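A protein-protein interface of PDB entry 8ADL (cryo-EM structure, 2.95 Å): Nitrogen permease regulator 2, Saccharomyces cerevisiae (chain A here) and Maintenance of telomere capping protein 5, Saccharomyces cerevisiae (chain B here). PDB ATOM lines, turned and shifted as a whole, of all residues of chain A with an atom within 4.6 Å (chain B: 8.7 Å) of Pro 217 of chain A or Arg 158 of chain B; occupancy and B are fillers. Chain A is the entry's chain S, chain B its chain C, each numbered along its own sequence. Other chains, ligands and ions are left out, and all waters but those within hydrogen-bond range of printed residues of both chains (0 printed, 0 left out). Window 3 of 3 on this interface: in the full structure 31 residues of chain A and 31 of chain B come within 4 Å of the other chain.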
ATOM      1  N   ARG A 203     -27.790  27.139 -34.312  1.00  0.00           N
ATOM      2  CA  ARG A 203     -27.196  27.358 -32.999  1.00  0.00           C
ATOM      3  C   ARG A 203     -26.404  28.660 -32.950  1.00  0.00           C
ATOM      4  O   ARG A 203     -26.515  29.411 -31.977  1.00  0.00           O
ATOM      5  CB  ARG A 203     -26.311  26.175 -32.614  1.00  0.00           C
ATOM      6  CG  ARG A 203     -27.060  24.963 -32.088  1.00  0.00           C
ATOM      7  CD  ARG A 203     -27.503  25.190 -30.648  1.00  0.00           C
ATOM      8  NE  ARG A 203     -26.381  25.218 -29.717  1.00  0.00           N
ATOM      9  CZ  ARG A 203     -25.776  24.147 -29.222  1.00  0.00           C
ATOM     10  NH1 ARG A 203     -26.154  22.923 -29.551  1.00  0.00           N
ATOM     11  NH2 ARG A 203     -24.762  24.308 -28.377  1.00  0.00           N
ATOM     12  N   LEU A 215     -21.059  28.176 -27.572  1.00  0.00           N
ATOM     13  CA  LEU A 215     -20.121  27.052 -27.449  1.00  0.00           C
ATOM     14  C   LEU A 215     -20.806  25.866 -28.128  1.00  0.00           C
ATOM     15  O   LEU A 215     -21.580  25.138 -27.500  1.00  0.00           O
ATOM     16  CB  LEU A 215     -19.765  26.759 -25.996  1.00  0.00           C
ATOM     17  CG  LEU A 215     -18.544  25.878 -25.713  1.00  0.00           C
ATOM     18  CD1 LEU A 215     -17.817  26.366 -24.472  1.00  0.00           C
ATOM     19  CD2 LEU A 215     -18.934  24.414 -25.553  1.00  0.00           C
ATOM     20  N   ILE A 216     -20.515  25.680 -29.409  1.00  0.00           N
ATOM     21  CA  ILE A 216     -21.206  24.722 -30.260  1.00  0.00           C
ATOM     22  C   ILE A 216     -20.199  23.691 -30.754  1.00  0.00           C
ATOM     23  O   ILE A 216     -19.395  23.970 -31.643  1.00  0.00           O
ATOM     24  CB  ILE A 216     -21.902  25.425 -31.440  1.00  0.00           C
ATOM     25  CG1 ILE A 216     -22.819  26.530 -30.917  1.00  0.00           C
ATOM     26  CG2 ILE A 216     -22.686  24.422 -32.272  1.00  0.00           C
ATOM     27  CD1 ILE A 216     -23.044  27.637 -31.895  1.00  0.00           C
ATOM     28  N   PRO A 217     -20.208  22.481 -30.190  1.00  0.00           N
ATOM     29  CA  PRO A 217     -19.251  21.455 -30.631  1.00  0.00           C
ATOM     30  C   PRO A 217     -19.619  20.915 -32.006  1.00  0.00           C
ATOM     31  O   PRO A 217     -20.762  20.521 -32.249  1.00  0.00           O
ATOM     32  CB  PRO A 217     -19.364  20.368 -29.552  1.00  0.00           C
ATOM     33  CG  PRO A 217     -20.158  20.986 -28.431  1.00  0.00           C
ATOM     34  CD  PRO A 217     -21.031  22.017 -29.064  1.00  0.00           C
ATOM     35  N   ILE A 218     -18.636  20.899 -32.904  1.00  0.00           N
ATOM     36  CA  ILE A 218     -18.821  20.384 -34.258  1.00  0.00           C
ATOM     37  C   ILE A 218     -18.073  19.082 -34.507  1.00  0.00           C
ATOM     38  O   ILE A 218     -18.348  18.415 -35.519  1.00  0.00           O
ATOM     39  CB  ILE A 218     -18.431  21.432 -35.322  1.00  0.00           C
ATOM     40  CG1 ILE A 218     -16.925  21.696 -35.290  1.00  0.00           C
ATOM     41  CG2 ILE A 218     -19.215  22.720 -35.111  1.00  0.00           C
ATOM     42  CD1 ILE A 218     -16.479  22.750 -36.272  1.00  0.00           C
ATOM     43  N   ASP A 219     -17.148  18.698 -33.633  1.00  0.00           N
ATOM     44  CA  ASP A 219     -16.387  17.464 -33.788  1.00  0.00           C
ATOM     45  C   ASP A 219     -16.051  16.929 -32.402  1.00  0.00           C
ATOM     46  O   ASP A 219     -16.611  17.370 -31.394  1.00  0.00           O
ATOM     47  CB  ASP A 219     -15.115  17.696 -34.615  1.00  0.00           C
ATOM     48  CG  ASP A 219     -15.350  17.567 -36.104  1.00  0.00           C
ATOM     49  OD1 ASP A 219     -16.169  16.716 -36.511  1.00  0.00           O
ATOM     50  OD2 ASP A 219     -14.700  18.308 -36.868  1.00  0.00           O
ATOM     51  N   GLU A 220     -15.124  15.972 -32.351  1.00  0.00           N
ATOM     52  CA  GLU A 220     -14.642  15.453 -31.079  1.00  0.00           C
ATOM     53  C   GLU A 220     -13.549  16.318 -30.468  1.00  0.00           C
ATOM     54  O   GLU A 220     -13.172  16.088 -29.314  1.00  0.00           O
ATOM     55  CB  GLU A 220     -14.123  14.023 -31.251  1.00  0.00           C
ATOM     56  CG  GLU A 220     -15.142  13.047 -31.817  1.00  0.00           C
ATOM     57  CD  GLU A 220     -14.972  12.825 -33.308  1.00  0.00           C
ATOM     58  OE1 GLU A 220     -13.902  13.181 -33.847  1.00  0.00           O
ATOM     59  OE2 GLU A 220     -15.908  12.294 -33.942  1.00  0.00           O
ATOM     60  N   ASN A 222     -13.267  19.888 -31.882  1.00  0.00           N
ATOM     61  CA  ASN A 222     -13.525  21.208 -32.435  1.00  0.00           C
ATOM     62  C   ASN A 222     -14.866  21.730 -31.947  1.00  0.00           C
ATOM     63  O   ASN A 222     -15.848  20.984 -31.871  1.00  0.00           O
ATOM     64  CB  ASN A 222     -13.513  21.181 -33.967  1.00  0.00           C
ATOM     65  CG  ASN A 222     -12.120  21.031 -34.537  1.00  0.00           C
ATOM     66  OD1 ASN A 222     -11.275  21.909 -34.374  1.00  0.00           O
ATOM     67  ND2 ASN A 222     -11.872  19.913 -35.210  1.00  0.00           N
ATOM     68  N   ALA A 223     -14.895  23.018 -31.616  1.00  0.00           N
ATOM     69  CA  ALA A 223     -16.110  23.684 -31.183  1.00  0.00           C
ATOM     70  C   ALA A 223     -16.047  25.141 -31.613  1.00  0.00           C
ATOM     71  O   ALA A 223     -14.963  25.710 -31.773  1.00  0.00           O
ATOM     72  CB  ALA A 223     -16.304  23.585 -29.664  1.00  0.00           C
ATOM     73  N   VAL B 135     -23.013  28.918 -20.715  1.00  0.00           N
ATOM     74  CA  VAL B 135     -22.354  28.523 -21.955  1.00  0.00           C
ATOM     75  C   VAL B 135     -21.010  27.840 -21.701  1.00  0.00           C
ATOM     76  O   VAL B 135     -20.558  27.037 -22.527  1.00  0.00           O
ATOM     77  CB  VAL B 135     -22.209  29.766 -22.862  1.00  0.00           C
ATOM     78  CG1 VAL B 135     -21.771  29.395 -24.279  1.00  0.00           C
ATOM     79  CG2 VAL B 135     -23.513  30.546 -22.905  1.00  0.00           C
ATOM     80  N   ASP B 136     -20.380  28.080 -20.546  1.00  0.00           N
ATOM     81  CA  ASP B 136     -19.064  27.515 -20.254  1.00  0.00           C
ATOM     82  C   ASP B 136     -19.111  26.058 -19.775  1.00  0.00           C
ATOM     83  O   ASP B 136     -18.117  25.592 -19.200  1.00  0.00           O
ATOM     84  CB  ASP B 136     -18.330  28.388 -19.227  1.00  0.00           C
ATOM     85  CG  ASP B 136     -18.913  28.279 -17.830  1.00  0.00           C
ATOM     86  OD1 ASP B 136     -20.135  28.071 -17.700  1.00  0.00           O
ATOM     87  OD2 ASP B 136     -18.142  28.403 -16.856  1.00  0.00           O
ATOM     88  N   THR B 137     -20.221  25.355 -20.028  1.00  0.00           N
ATOM     89  CA  THR B 137     -20.433  23.946 -19.671  1.00  0.00           C
ATOM     90  C   THR B 137     -20.273  23.723 -18.165  1.00  0.00           C
ATOM     91  O   THR B 137     -19.399  22.987 -17.704  1.00  0.00           O
ATOM     92  CB  THR B 137     -19.515  23.010 -20.472  1.00  0.00           C
ATOM     93  OG1 THR B 137     -18.181  23.074 -19.950  1.00  0.00           O
ATOM     94  CG2 THR B 137     -19.505  23.383 -21.954  1.00  0.00           C
ATOM     95  N   TYR B 138     -21.148  24.376 -17.404  1.00  0.00           N
ATOM     96  CA  TYR B 138     -21.190  24.221 -15.957  1.00  0.00           C
ATOM     97  C   TYR B 138     -22.615  24.451 -15.480  1.00  0.00           C
ATOM     98  O   TYR B 138     -23.302  25.352 -15.967  1.00  0.00           O
ATOM     99  CB  TYR B 138     -20.242  25.194 -15.247  1.00  0.00           C
ATOM    100  CG  TYR B 138     -18.807  24.726 -15.191  1.00  0.00           C
ATOM    101  CD1 TYR B 138     -18.408  23.765 -14.272  1.00  0.00           C
ATOM    102  CD2 TYR B 138     -17.851  25.249 -16.052  1.00  0.00           C
ATOM    103  CE1 TYR B 138     -17.100  23.334 -14.216  1.00  0.00           C
ATOM    104  CE2 TYR B 138     -16.540  24.822 -16.005  1.00  0.00           C
ATOM    105  CZ  TYR B 138     -16.173  23.867 -15.083  1.00  0.00           C
ATOM    106  OH  TYR B 138     -14.871  23.440 -15.029  1.00  0.00           O
ATOM    107  N   SER B 155     -20.934  19.398 -14.414  1.00  0.00           N
ATOM    108  CA  SER B 155     -20.609  19.804 -15.772  1.00  0.00           C
ATOM    109  C   SER B 155     -20.881  18.651 -16.728  1.00  0.00           C
ATOM    110  O   SER B 155     -20.900  17.481 -16.336  1.00  0.00           O
ATOM    111  CB  SER B 155     -19.149  20.257 -15.885  1.00  0.00           C
ATOM    112  OG  SER B 155     -18.805  20.545 -17.229  1.00  0.00           O
ATOM    113  N   SER B 156     -21.094  19.001 -17.999  1.00  0.00           N
ATOM    114  CA  SER B 156     -21.163  18.023 -19.078  1.00  0.00           C
ATOM    115  C   SER B 156     -19.863  17.905 -19.860  1.00  0.00           C
ATOM    116  O   SER B 156     -19.694  16.928 -20.600  1.00  0.00           O
ATOM    117  CB  SER B 156     -22.295  18.374 -20.049  1.00  0.00           C
ATOM    118  OG  SER B 156     -22.141  19.691 -20.547  1.00  0.00           O
ATOM    119  N   TRP B 157     -18.993  18.918 -19.763  1.00  0.00           N
ATOM    120  CA  TRP B 157     -17.624  18.964 -20.282  1.00  0.00           C
ATOM    121  C   TRP B 157     -17.513  19.003 -21.805  1.00  0.00           C
ATOM    122  O   TRP B 157     -16.407  19.150 -22.333  1.00  0.00           O
ATOM    123  CB  TRP B 157     -16.805  17.778 -19.757  1.00  0.00           C
ATOM    124  CG  TRP B 157     -16.923  17.542 -18.282  1.00  0.00           C
ATOM    125  CD1 TRP B 157     -17.606  16.531 -17.670  1.00  0.00           C
ATOM    126  CD2 TRP B 157     -16.330  18.317 -17.233  1.00  0.00           C
ATOM    127  NE1 TRP B 157     -17.482  16.633 -16.306  1.00  0.00           N
ATOM    128  CE2 TRP B 157     -16.702  17.719 -16.012  1.00  0.00           C
ATOM    129  CE3 TRP B 157     -15.524  19.459 -17.208  1.00  0.00           C
ATOM    130  CZ2 TRP B 157     -16.298  18.226 -14.779  1.00  0.00           C
ATOM    131  CZ3 TRP B 157     -15.123  19.960 -15.981  1.00  0.00           C
ATOM    132  CH2 TRP B 157     -15.512  19.344 -14.784  1.00  0.00           C
ATOM    133  N   ARG B 158     -18.626  18.877 -22.527  1.00  0.00           N
ATOM    134  CA  ARG B 158     -18.580  18.913 -23.985  1.00  0.00           C
ATOM    135  C   ARG B 158     -19.394  20.047 -24.584  1.00  0.00           C
ATOM    136  O   ARG B 158     -18.858  20.839 -25.367  1.00  0.00           O
ATOM    137  CB  ARG B 158     -19.056  17.567 -24.559  1.00  0.00           C
ATOM    138  CG  ARG B 158     -17.938  16.576 -24.843  1.00  0.00           C
ATOM    139  CD  ARG B 158     -16.846  17.206 -25.697  1.00  0.00           C
ATOM    140  NE  ARG B 158     -15.663  16.360 -25.793  1.00  0.00           N
ATOM    141  CZ  ARG B 158     -15.454  15.469 -26.754  1.00  0.00           C
ATOM    142  NH1 ARG B 158     -16.334  15.281 -27.725  1.00  0.00           N
ATOM    143  NH2 ARG B 158     -14.334  14.752 -26.743  1.00  0.00           N
ATOM    144  N   SER B 159     -20.675  20.155 -24.239  1.00  0.00           N
ATOM    145  CA  SER B 159     -21.587  21.059 -24.921  1.00  0.00           C
ATOM    146  C   SER B 159     -22.164  22.080 -23.952  1.00  0.00           C
ATOM    147  O   SER B 159     -22.356  21.797 -22.765  1.00  0.00           O
ATOM    148  CB  SER B 159     -22.731  20.292 -25.594  1.00  0.00           C
ATOM    149  OG  SER B 159     -23.706  21.185 -26.098  1.00  0.00           O
ATOM    150  N   ALA B 160     -22.426  23.278 -24.473  1.00  0.00           N
ATOM    151  CA  ALA B 160     -22.993  24.350 -23.668  1.00  0.00           C
ATOM    152  C   ALA B 160     -24.424  24.022 -23.264  1.00  0.00           C
ATOM    153  O   ALA B 160     -25.198  23.465 -24.048  1.00  0.00           O
ATOM    154  CB  ALA B 160     -22.958  25.669 -24.436  1.00  0.00           C
ATOM    155  N   ALA B 161     -24.772  24.365 -22.027  1.00  0.00           N
ATOM    156  CA  ALA B 161     -26.105  24.088 -21.518  1.00  0.00           C
ATOM    157  C   ALA B 161     -27.128  25.042 -22.124  1.00  0.00           C
ATOM    158  O   ALA B 161     -26.805  26.162 -22.527  1.00  0.00           O
ATOM    159  CB  ALA B 161     -26.129  24.201 -19.996  1.00  0.00           C
ATOM    160  N   HIS B 178     -27.603  19.765 -22.756  1.00  0.00           N
ATOM    161  CA  HIS B 178     -26.336  20.255 -23.297  1.00  0.00           C
ATOM    162  C   HIS B 178     -26.239  19.810 -24.753  1.00  0.00           C
ATOM    163  O   HIS B 178     -25.721  18.731 -25.050  1.00  0.00           O
ATOM    164  CB  HIS B 178     -25.149  19.740 -22.482  1.00  0.00           C
ATOM    165  CG  HIS B 178     -25.190  20.124 -21.035  1.00  0.00           C
ATOM    166  ND1 HIS B 178     -24.320  21.040 -20.485  1.00  0.00           N
ATOM    167  CD2 HIS B 178     -25.982  19.703 -20.021  1.00  0.00           C
ATOM    168  CE1 HIS B 178     -24.577  21.170 -19.196  1.00  0.00           C
ATOM    169  NE2 HIS B 178     -25.583  20.372 -18.890  1.00  0.00           N
ATOM    170  N   GLY B 179     -26.737  20.647 -25.660  1.00  0.00           N
ATOM    171  CA  GLY B 179     -26.715  20.322 -27.072  1.00  0.00           C
ATOM    172  C   GLY B 179     -27.724  19.255 -27.436  1.00  0.00           C
ATOM    173  O   GLY B 179     -28.932  19.459 -27.290  1.00  0.00           O
ATOM    174  N   ASN B 180     -27.238  18.107 -27.899  1.00  0.00           N
ATOM    175  CA  ASN B 180     -28.108  17.009 -28.289  1.00  0.00           C
ATOM    176  C   ASN B 180     -28.467  16.102 -27.121  1.00  0.00           C
ATOM    177  O   ASN B 180     -29.305  15.208 -27.284  1.00  0.00           O
ATOM    178  CB  ASN B 180     -27.445  16.172 -29.388  1.00  0.00           C
ATOM    179  CG  ASN B 180     -26.799  17.025 -30.463  1.00  0.00           C
ATOM    180  OD1 ASN B 180     -27.328  18.066 -30.848  1.00  0.00           O
ATOM    181  ND2 ASN B 180     -25.645  16.587 -30.952  1.00  0.00           N
ATOM    182  N   ASP B 181     -27.858  16.309 -25.957  1.00  0.00           N
ATOM    183  CA  ASP B 181     -27.956  15.389 -24.837  1.00  0.00           C
ATOM    184  C   ASP B 181     -28.659  16.063 -23.668  1.00  0.00           C
ATOM    185  O   ASP B 181     -28.558  17.279 -23.477  1.00  0.00           O
ATOM    186  CB  ASP B 181     -26.569  14.904 -24.399  1.00  0.00           C
ATOM    187  CG  ASP B 181     -25.781  14.289 -25.539  1.00  0.00           C
ATOM    188  OD1 ASP B 181     -26.405  13.703 -26.448  1.00  0.00           O
ATOM    189  OD2 ASP B 181     -24.537  14.398 -25.528  1.00  0.00           O
ATOM    190  N   PHE B 183     -28.883  15.550 -19.517  1.00  0.00           N
ATOM    191  CA  PHE B 183     -28.301  14.896 -18.353  1.00  0.00           C
ATOM    192  C   PHE B 183     -29.127  15.226 -17.119  1.00  0.00           C
ATOM    193  O   PHE B 183     -29.464  16.391 -16.887  1.00  0.00           O
ATOM    194  CB  PHE B 183     -26.850  15.337 -18.153  1.00  0.00           C
ATOM    195  CG  PHE B 183     -25.947  14.998 -19.304  1.00  0.00           C
ATOM    196  CD1 PHE B 183     -25.464  13.709 -19.470  1.00  0.00           C
ATOM    197  CD2 PHE B 183     -25.580  15.970 -20.222  1.00  0.00           C
ATOM    198  CE1 PHE B 183     -24.630  13.396 -20.530  1.00  0.00           C
ATOM    199  CE2 PHE B 183     -24.749  15.664 -21.284  1.00  0.00           C
ATOM    200  CZ  PHE B 183     -24.274  14.375 -21.438  1.00  0.00           C
ATOM    201  N   SER B 203     -30.110  19.670 -31.747  1.00  0.00           N
ATOM    202  CA  SER B 203     -29.800  20.211 -30.431  1.00  0.00           C
ATOM    203  C   SER B 203     -31.075  20.449 -29.633  1.00  0.00           C
ATOM    204  O   SER B 203     -32.030  21.050 -30.133  1.00  0.00           O
ATOM    205  CB  SER B 203     -29.010  21.511 -30.566  1.00  0.00           C
ATOM    206  OG  SER B 203     -27.641  21.252 -30.824  1.00  0.00           O
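The backbone carbonyl oxygen (O) of Glu 220 of chain A lies within hydrogen-bond range of the guanidinium group (NH2) of Arg 158 of chain B.
The side-chain hydroxyl (OG) of Ser 203 of chain B sits at hydrogen-bond distance from the guanidinium group (NH1) of Arg 203 of chain A (2.6 Å).
The backbone NH (N) of Gly 179 of chain B sits at hydrogen-bond distance from the side-chain hydroxyl (OG) of Ser 159 of chain B (3.1 Å).
A ring nitrogen (ND1) of His 178 of chain B is in hydrogen-bond range of the backbone carbonyl oxygen (O) of Ser 159 of chain B, 3.1 Å away.
The guanidinium group of Arg 203 of chain A is in hydrogen-bond range of the backbone carbonyl oxygen of Leu 215 of chain A (3.4 Å).
The side-chain hydroxyl (OG) of Ser 156 of chain B is in hydrogen-bond range of the backbone carbonyl oxygen (O) of Ser 159 of chain B.
OG of Ser 203 of chain B lies within hydrogen-bond range of OD1 of Asn 180 of chain B (3.2 Å).
The backbone carbonyl oxygen (O) of Thr 137 of chain B is in hydrogen-bond range of the side-chain hydroxyl (OG) of Ser 155 of chain B, 2.6 Å away.
Of chain B, only Arg 158 (3.3 Å) and Ser 159 (3.8 Å) come within 4 Å of Pro 217 of chain A.
Arg 158 of chain B touches three residues of chain A.
Of the printed residues of chain B, Leu 215 of chain A touches Val 135, Thr 137, Arg 158 and Ala 160.
Of the printed residues of chain A, Ala 160 of chain B touches Leu 215 (3.4 Å).
Of the printed residues of chain A, Thr 137 of chain B touches Leu 215 (3.8 Å).
Ala 223 of chain A touches none of the printed residues of chain B.
Asn 222 of chain A touches none of the printed residues of chain B.
The nearest residue of chain B that does not touch Pro 217 of chain A is Ala 160 of chain B (5.0 Å).
The nearest residue of chain A that does not touch Arg 158 of chain B is Asp 219 of chain A (4.2 Å).
The nearest printed residue of chain B that does not touch Glu 220 of chain A is Trp 157 of chain B (8.3 Å).
Hydrophobic or aromatic side chains of chain B that line the printed part of chain A: Val 135 and Ala 160.
Printed residues of chain A that touch a printed residue of chain B: Arg 203, Leu 215, Pro 217 and Glu 220.
Hydrophobic or aromatic side chains of chain A that line the printed part of chain B: Leu 215 and Pro 217.
Among the printed residues, 9 pairs touch across the chains.
Arg 203 of chain A touches Gly 179 of chain B.
Leu 215 of chain A touches Val 135 of chain B (CD1 to O, 3.4 Å).
CD2 of Leu 215 of chain A touches CG2 of Thr 137 of chain B, 3.8 Å away.
CD2 of Leu 215 of chain A touches O of Arg 158 of chain B, at 3.6 Å.
Ala 160 of chain B touches Leu 215 of chain A.
Arg 158 of chain B touches Pro 217 of chain A.
Ser 159 of chain B touches Pro 217 of chain A.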
